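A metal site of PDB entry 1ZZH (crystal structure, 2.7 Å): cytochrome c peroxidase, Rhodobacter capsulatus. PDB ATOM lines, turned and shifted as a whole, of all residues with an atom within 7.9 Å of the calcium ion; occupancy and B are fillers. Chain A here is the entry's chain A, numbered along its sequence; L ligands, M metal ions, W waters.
N of His 264 lies within hydrogen-bond range of O3 of the ligand, 2.7 Å away. The backbone NH (N) of Phe 263 sits at hydrogen-bond distance from an oxygen (O1) of the ligand (2.7 Å). ND1 of His 264 is in hydrogen-bond range of O4 of the ligand (2.8 Å).
The backbone carbonyl oxygen (O) of Leu 68 sits at hydrogen-bond distance from the side-chain amide nitrogen (ND2) of Asn 82, 2.8 Å away. The backbone carbonyl oxygen (O) of Glu 69 sits at hydrogen-bond distance from the side-chain amide nitrogen (ND2) of Asn 82 (2.8 Å). OG1 of Thr 259 lies close to O of Ile 256, 3.3 Å away. N of Asn 82 sits at hydrogen-bond distance from O of His 264. The backbone carbonyl oxygen (O) of Asn 82 lies within hydrogen-bond range of the indole nitrogen (NE1) of Trp 97, at 2.8 Å.
Of the 21 residues printed, 3 come within 4 Å of the calcium ion. The nearest printed residue that does not touch the calcium ion is Tyr 262 (4.04 Å).
The calcium ion is bound by water W1 (2.2 Å), O of Pro 261 (2.3 Å), water W2 (2.3 Å), OD1 of Asn 82 (2.4 Å) and O of Thr 259 (2.4 Å). The calcium ion has five donor atoms within binding distance.
Water W1 bridges the backbone carbonyl oxygen of Ala 260 (2.9 Å) and the side-chain amide nitrogen of Asn 82 (3.2 Å).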
ATOM      1  N   VAL A  65     -14.620 -22.831  34.032  1.00  0.00           N
ATOM      2  CA  VAL A  65     -15.181 -23.881  33.191  1.00  0.00           C
ATOM      3  C   VAL A  65     -14.856 -25.221  33.873  1.00  0.00           C
ATOM      4  O   VAL A  65     -14.344 -25.233  34.986  1.00  0.00           O
ATOM      5  CB  VAL A  65     -14.558 -23.798  31.766  1.00  0.00           C
ATOM      6  CG1 VAL A  65     -15.001 -24.978  30.899  1.00  0.00           C
ATOM      7  CG2 VAL A  65     -15.016 -22.504  31.092  1.00  0.00           C
ATOM      8  N   ASP A  66     -15.180 -26.351  33.229  1.00  0.00           N
ATOM      9  CA  ASP A  66     -14.889 -27.663  33.797  1.00  0.00           C
ATOM     10  C   ASP A  66     -13.825 -28.429  33.008  1.00  0.00           C
ATOM     11  O   ASP A  66     -13.410 -29.509  33.419  1.00  0.00           O
ATOM     12  CB  ASP A  66     -16.159 -28.527  33.902  1.00  0.00           C
ATOM     13  CG  ASP A  66     -16.772 -28.862  32.549  1.00  0.00           C
ATOM     14  OD1 ASP A  66     -16.204 -28.465  31.492  1.00  0.00           O
ATOM     15  OD2 ASP A  66     -17.839 -29.522  32.536  1.00  0.00           O
ATOM     16  N   GLY A  67     -13.382 -27.855  31.888  1.00  0.00           N
ATOM     17  CA  GLY A  67     -12.354 -28.494  31.075  1.00  0.00           C
ATOM     18  C   GLY A  67     -12.766 -29.758  30.347  1.00  0.00           C
ATOM     19  O   GLY A  67     -11.910 -30.509  29.892  1.00  0.00           O
ATOM     20  N   LEU A  68     -14.067 -29.987  30.219  1.00  0.00           N
ATOM     21  CA  LEU A  68     -14.582 -31.168  29.551  1.00  0.00           C
ATOM     22  C   LEU A  68     -15.244 -30.785  28.230  1.00  0.00           C
ATOM     23  O   LEU A  68     -15.626 -29.634  28.023  1.00  0.00           O
ATOM     24  CB  LEU A  68     -15.607 -31.867  30.453  1.00  0.00           C
ATOM     25  CG  LEU A  68     -15.158 -32.135  31.888  1.00  0.00           C
ATOM     26  CD1 LEU A  68     -16.265 -32.874  32.644  1.00  0.00           C
ATOM     27  CD2 LEU A  68     -13.857 -32.938  31.872  1.00  0.00           C
ATOM     28  N   GLU A  69     -15.369 -31.758  27.324  1.00  0.00           N
ATOM     29  CA  GLU A  69     -15.992 -31.483  26.038  1.00  0.00           C
ATOM     30  C   GLU A  69     -17.422 -30.971  26.292  1.00  0.00           C
ATOM     31  O   GLU A  69     -17.834 -29.953  25.754  1.00  0.00           O
ATOM     32  CB  GLU A  69     -16.028 -32.730  25.148  1.00  0.00           C
ATOM     33  CG  GLU A  69     -14.655 -33.337  24.846  1.00  0.00           C
ATOM     34  CD  GLU A  69     -14.612 -34.002  23.475  1.00  0.00           C
ATOM     35  OE1 GLU A  69     -15.550 -34.750  23.136  1.00  0.00           O
ATOM     36  OE2 GLU A  69     -13.618 -33.774  22.731  1.00  0.00           O
ATOM     37  N   ASN A  82     -20.856 -27.713  26.021  1.00  0.00           N
ATOM     38  CA  ASN A  82     -19.601 -27.319  26.628  1.00  0.00           C
ATOM     39  C   ASN A  82     -19.869 -26.175  27.603  1.00  0.00           C
ATOM     40  O   ASN A  82     -20.336 -25.106  27.204  1.00  0.00           O
ATOM     41  CB  ASN A  82     -18.606 -26.861  25.565  1.00  0.00           C
ATOM     42  CG  ASN A  82     -17.227 -26.552  26.160  1.00  0.00           C
ATOM     43  OD1 ASN A  82     -16.892 -25.395  26.440  1.00  0.00           O
ATOM     44  ND2 ASN A  82     -16.428 -27.594  26.341  1.00  0.00           N
ATOM     45  N   ALA A  83     -19.567 -26.419  28.865  1.00  0.00           N
ATOM     46  CA  ALA A  83     -19.775 -25.423  29.912  1.00  0.00           C
ATOM     47  C   ALA A  83     -18.967 -24.142  29.721  1.00  0.00           C
ATOM     48  O   ALA A  83     -17.723 -24.162  29.645  1.00  0.00           O
ATOM     49  CB  ALA A  83     -19.479 -26.031  31.268  1.00  0.00           C
ATOM     50  N   PRO A  84     -19.651 -22.998  29.619  1.00  0.00           N
ATOM     51  CA  PRO A  84     -19.039 -21.693  29.445  1.00  0.00           C
ATOM     52  C   PRO A  84     -18.524 -21.183  30.795  1.00  0.00           C
ATOM     53  O   PRO A  84     -19.011 -21.587  31.856  1.00  0.00           O
ATOM     54  CB  PRO A  84     -20.187 -20.850  28.910  1.00  0.00           C
ATOM     55  CG  PRO A  84     -21.355 -21.437  29.631  1.00  0.00           C
ATOM     56  CD  PRO A  84     -21.111 -22.905  29.461  1.00  0.00           C
ATOM     57  N   THR A  85     -17.537 -20.294  30.745  1.00  0.00           N
ATOM     58  CA  THR A  85     -16.960 -19.746  31.961  1.00  0.00           C
ATOM     59  C   THR A  85     -17.967 -18.894  32.723  1.00  0.00           C
ATOM     60  O   THR A  85     -18.789 -18.212  32.118  1.00  0.00           O
ATOM     61  CB  THR A  85     -15.745 -18.872  31.660  1.00  0.00           C
ATOM     62  OG1 THR A  85     -15.165 -18.404  32.889  1.00  0.00           O
ATOM     63  CG2 THR A  85     -16.144 -17.673  30.823  1.00  0.00           C
ATOM     64  N   TRP A  97     -26.774 -21.474  25.162  1.00  0.00           N
ATOM     65  CA  TRP A  97     -25.990 -21.986  24.062  1.00  0.00           C
ATOM     66  C   TRP A  97     -26.722 -22.035  22.732  1.00  0.00           C
ATOM     67  O   TRP A  97     -26.168 -21.666  21.692  1.00  0.00           O
ATOM     68  CB  TRP A  97     -25.509 -23.398  24.385  1.00  0.00           C
ATOM     69  CG  TRP A  97     -24.036 -23.498  24.517  1.00  0.00           C
ATOM     70  CD1 TRP A  97     -23.350 -24.043  25.554  1.00  0.00           C
ATOM     71  CD2 TRP A  97     -23.056 -23.033  23.571  1.00  0.00           C
ATOM     72  NE1 TRP A  97     -21.992 -23.951  25.322  1.00  0.00           N
ATOM     73  CE2 TRP A  97     -21.786 -23.342  24.118  1.00  0.00           C
ATOM     74  CE3 TRP A  97     -23.130 -22.400  22.332  1.00  0.00           C
ATOM     75  CZ2 TRP A  97     -20.582 -23.014  23.452  1.00  0.00           C
ATOM     76  CZ3 TRP A  97     -21.923 -22.084  21.659  1.00  0.00           C
ATOM     77  CH2 TRP A  97     -20.672 -22.397  22.236  1.00  0.00           C
ATOM     78  N   ILE A 256     -10.872 -16.961  26.906  1.00  0.00           N
ATOM     79  CA  ILE A 256     -10.980 -18.161  26.094  1.00  0.00           C
ATOM     80  C   ILE A 256      -9.699 -19.001  26.136  1.00  0.00           C
ATOM     81  O   ILE A 256      -9.758 -20.224  26.029  1.00  0.00           O
ATOM     82  CB  ILE A 256     -11.291 -17.809  24.627  1.00  0.00           C
ATOM     83  CG1 ILE A 256     -11.614 -19.090  23.864  1.00  0.00           C
ATOM     84  CG2 ILE A 256     -10.121 -17.094  23.990  1.00  0.00           C
ATOM     85  CD1 ILE A 256     -12.123 -18.860  22.470  1.00  0.00           C
ATOM     86  N   LEU A 258      -8.218 -19.911  28.461  1.00  0.00           N
ATOM     87  CA  LEU A 258      -8.326 -20.809  29.603  1.00  0.00           C
ATOM     88  C   LEU A 258      -9.556 -21.705  29.557  1.00  0.00           C
ATOM     89  O   LEU A 258      -9.721 -22.568  30.426  1.00  0.00           O
ATOM     90  CB  LEU A 258      -8.415 -19.995  30.905  1.00  0.00           C
ATOM     91  CG  LEU A 258      -7.508 -18.791  31.117  1.00  0.00           C
ATOM     92  CD1 LEU A 258      -7.876 -18.101  32.414  1.00  0.00           C
ATOM     93  CD2 LEU A 258      -6.070 -19.239  31.130  1.00  0.00           C
ATOM     94  N   THR A 259     -10.425 -21.505  28.572  1.00  0.00           N
ATOM     95  CA  THR A 259     -11.652 -22.282  28.535  1.00  0.00           C
ATOM     96  C   THR A 259     -11.812 -23.368  27.471  1.00  0.00           C
ATOM     97  O   THR A 259     -12.910 -23.592  26.940  1.00  0.00           O
ATOM     98  CB  THR A 259     -12.863 -21.327  28.495  1.00  0.00           C
ATOM     99  OG1 THR A 259     -12.829 -20.552  27.300  1.00  0.00           O
ATOM    100  CG2 THR A 259     -12.829 -20.382  29.686  1.00  0.00           C
ATOM    101  N   ALA A 260     -10.716 -24.058  27.165  1.00  0.00           N
ATOM    102  CA  ALA A 260     -10.767 -25.159  26.195  1.00  0.00           C
ATOM    103  C   ALA A 260     -11.565 -26.294  26.850  1.00  0.00           C
ATOM    104  O   ALA A 260     -11.643 -26.380  28.073  1.00  0.00           O
ATOM    105  CB  ALA A 260      -9.366 -25.631  25.869  1.00  0.00           C
ATOM    106  N   PRO A 261     -12.181 -27.171  26.044  1.00  0.00           N
ATOM    107  CA  PRO A 261     -12.242 -27.180  24.582  1.00  0.00           C
ATOM    108  C   PRO A 261     -13.224 -26.126  24.113  1.00  0.00           C
ATOM    109  O   PRO A 261     -13.878 -25.462  24.930  1.00  0.00           O
ATOM    110  CB  PRO A 261     -12.707 -28.602  24.278  1.00  0.00           C
ATOM    111  CG  PRO A 261     -13.626 -28.888  25.422  1.00  0.00           C
ATOM    112  CD  PRO A 261     -12.862 -28.354  26.614  1.00  0.00           C
ATOM    113  N   TYR A 262     -13.357 -25.974  22.793  1.00  0.00           N
ATOM    114  CA  TYR A 262     -14.232 -24.947  22.239  1.00  0.00           C
ATOM    115  C   TYR A 262     -15.455 -25.372  21.444  1.00  0.00           C
ATOM    116  O   TYR A 262     -15.563 -26.512  21.023  1.00  0.00           O
ATOM    117  CB  TYR A 262     -13.377 -23.985  21.412  1.00  0.00           C
ATOM    118  CG  TYR A 262     -12.135 -23.533  22.166  1.00  0.00           C
ATOM    119  CD1 TYR A 262     -10.867 -24.023  21.828  1.00  0.00           C
ATOM    120  CD2 TYR A 262     -12.232 -22.669  23.264  1.00  0.00           C
ATOM    121  CE1 TYR A 262      -9.730 -23.675  22.559  1.00  0.00           C
ATOM    122  CE2 TYR A 262     -11.106 -22.303  24.004  1.00  0.00           C
ATOM    123  CZ  TYR A 262      -9.853 -22.810  23.644  1.00  0.00           C
ATOM    124  OH  TYR A 262      -8.736 -22.449  24.358  1.00  0.00           O
ATOM    125  N   PHE A 263     -16.385 -24.429  21.264  1.00  0.00           N
ATOM    126  CA  PHE A 263     -17.652 -24.626  20.559  1.00  0.00           C
ATOM    127  C   PHE A 263     -18.623 -25.408  21.442  1.00  0.00           C
ATOM    128  O   PHE A 263     -18.211 -26.057  22.394  1.00  0.00           O
ATOM    129  CB  PHE A 263     -17.426 -25.307  19.196  1.00  0.00           C
ATOM    130  CG  PHE A 263     -16.577 -24.507  18.254  1.00  0.00           C
ATOM    131  CD1 PHE A 263     -15.448 -25.065  17.657  1.00  0.00           C
ATOM    132  CD2 PHE A 263     -16.865 -23.161  18.004  1.00  0.00           C
ATOM    133  CE1 PHE A 263     -14.628 -24.296  16.821  1.00  0.00           C
ATOM    134  CE2 PHE A 263     -16.063 -22.392  17.190  1.00  0.00           C
ATOM    135  CZ  PHE A 263     -14.935 -22.955  16.602  1.00  0.00           C
ATOM    136  N   HIS A 264     -19.925 -25.330  21.141  1.00  0.00           N
ATOM    137  CA  HIS A 264     -20.922 -26.012  21.963  1.00  0.00           C
ATOM    138  C   HIS A 264     -20.666 -27.490  22.215  1.00  0.00           C
ATOM    139  O   HIS A 264     -21.070 -28.023  23.247  1.00  0.00           O
ATOM    140  CB  HIS A 264     -22.311 -25.864  21.325  1.00  0.00           C
ATOM    141  CG  HIS A 264     -22.474 -26.662  20.077  1.00  0.00           C
ATOM    142  ND1 HIS A 264     -21.851 -26.338  18.892  1.00  0.00           N
ATOM    143  CD2 HIS A 264     -23.144 -27.826  19.853  1.00  0.00           C
ATOM    144  CE1 HIS A 264     -22.137 -27.262  17.988  1.00  0.00           C
ATOM    145  NE2 HIS A 264     -22.915 -28.165  18.544  1.00  0.00           N
ATOM    146  N   SER A 265     -19.996 -28.160  21.280  1.00  0.00           N
ATOM    147  CA  SER A 265     -19.713 -29.590  21.424  1.00  0.00           C
ATOM    148  C   SER A 265     -18.439 -29.828  22.208  1.00  0.00           C
ATOM    149  O   SER A 265     -18.226 -30.914  22.734  1.00  0.00           O
ATOM    150  CB  SER A 265     -19.569 -30.242  20.046  1.00  0.00           C
ATOM    151  OG  SER A 265     -18.539 -29.640  19.310  1.00  0.00           O
ATOM    152  N   GLY A 266     -17.598 -28.796  22.282  1.00  0.00           N
ATOM    153  CA  GLY A 266     -16.338 -28.915  23.005  1.00  0.00           C
ATOM    154  C   GLY A 266     -15.427 -29.930  22.348  1.00  0.00           C
ATOM    155  O   GLY A 266     -14.642 -30.602  23.025  1.00  0.00           O
ATOM    156  N   VAL A 268     -13.252 -29.137  19.664  1.00  0.00           N
ATOM    157  CA  VAL A 268     -11.992 -28.564  19.210  1.00  0.00           C
ATOM    158  C   VAL A 268     -11.215 -28.132  20.460  1.00  0.00           C
ATOM    159  O   VAL A 268     -11.698 -27.337  21.264  1.00  0.00           O
ATOM    160  CB  VAL A 268     -12.207 -27.349  18.261  1.00  0.00           C
ATOM    161  CG1 VAL A 268     -13.143 -27.743  17.097  1.00  0.00           C
ATOM    162  CG2 VAL A 268     -12.775 -26.187  19.033  1.00  0.00           C
HETATM  163 FE1  LIG L   1     -17.463 -16.984  16.137  1.00  0.00          FE
HETATM  164  C1  LIG L   1     -18.027 -19.425  18.394  1.00  0.00           C
HETATM  165  C2  LIG L   1     -14.173 -17.118  16.816  1.00  0.00           C
HETATM  166  C3  LIG L   1     -16.930 -14.776  13.642  1.00  0.00           C
HETATM  167  C4  LIG L   1     -20.800 -16.936  15.429  1.00  0.00           C
HETATM  168  N1  LIG L   1     -16.343 -18.000  17.378  1.00  0.00           N
HETATM  169  C5  LIG L   1     -16.736 -18.971  18.267  1.00  0.00           C
HETATM  170  C6  LIG L   1     -15.610 -19.475  19.048  1.00  0.00           C
HETATM  171  C7  LIG L   1     -14.529 -18.819  18.588  1.00  0.00           C
HETATM  172  C8  LIG L   1     -14.991 -17.918  17.542  1.00  0.00           C
HETATM  173  C9  LIG L   1     -13.075 -19.009  19.059  1.00  0.00           C
HETATM  174  C10 LIG L   1     -15.683 -20.555  20.149  1.00  0.00           C
HETATM  175  C11 LIG L   1     -15.786 -19.896  21.534  1.00  0.00           C
HETATM  176  C12 LIG L   1     -15.841 -20.863  22.724  1.00  0.00           C
HETATM  177  O1  LIG L   1     -15.814 -22.100  22.560  1.00  0.00           O
HETATM  178  O2  LIG L   1     -15.897 -20.364  23.863  1.00  0.00           O
HETATM  179  N2  LIG L   1     -15.889 -16.130  15.399  1.00  0.00           N
HETATM  180  C13 LIG L   1     -14.564 -16.287  15.795  1.00  0.00           C
HETATM  181  C14 LIG L   1     -13.632 -15.555  14.972  1.00  0.00           C
HETATM  182  C15 LIG L   1     -14.428 -14.945  14.007  1.00  0.00           C
HETATM  183  C16 LIG L   1     -15.813 -15.262  14.340  1.00  0.00           C
HETATM  184  C17 LIG L   1     -12.086 -15.548  15.137  1.00  0.00           C
HETATM  185  C18 LIG L   1     -13.934 -14.103  12.824  1.00  0.00           C
HETATM  186  C19 LIG L   1     -13.096 -14.847  11.784  1.00  0.00           C
HETATM  187  N3  LIG L   1     -18.629 -16.013  14.867  1.00  0.00           N
HETATM  188  C20 LIG L   1     -18.257 -15.106  13.905  1.00  0.00           C
HETATM  189  C21 LIG L   1     -19.411 -14.571  13.174  1.00  0.00           C
HETATM  190  C22 LIG L   1     -20.486 -15.200  13.695  1.00  0.00           C
HETATM  191  C23 LIG L   1     -19.991 -16.100  14.722  1.00  0.00           C
HETATM  192  C24 LIG L   1     -19.346 -13.517  12.057  1.00  0.00           C
HETATM  193  C25 LIG L   1     -21.977 -15.042  13.295  1.00  0.00           C
HETATM  194  C26 LIG L   1     -22.399 -15.282  11.853  1.00  0.00           C
HETATM  195  N4  LIG L   1     -19.083 -17.964  16.754  1.00  0.00           N
HETATM  196  C27 LIG L   1     -20.384 -17.828  16.360  1.00  0.00           C
HETATM  197  C28 LIG L   1     -21.278 -18.778  16.994  1.00  0.00           C
HETATM  198  C29 LIG L   1     -20.474 -19.516  17.819  1.00  0.00           C
HETATM  199  C30 LIG L   1     -19.138 -18.964  17.683  1.00  0.00           C
HETATM  200  C31 LIG L   1     -22.798 -18.908  16.752  1.00  0.00           C
HETATM  201  C32 LIG L   1     -20.872 -20.698  18.716  1.00  0.00           C
HETATM  202  C33 LIG L   1     -21.405 -21.925  17.940  1.00  0.00           C
HETATM  203  C34 LIG L   1     -20.709 -23.256  18.214  1.00  0.00           C
HETATM  204  O3  LIG L   1     -20.062 -23.417  19.268  1.00  0.00           O
HETATM  205  O4  LIG L   1     -20.840 -24.187  17.378  1.00  0.00           O
HETATM  206 CA    CA M   1     -15.089 -23.923  26.048  1.00  0.00          CA
HETATM  207  O   HOH W   1     -14.299 -25.449  27.488  1.00  0.00           O
HETATM  208  O   HOH W   2     -15.932 -22.978  27.996  1.00  0.00           O
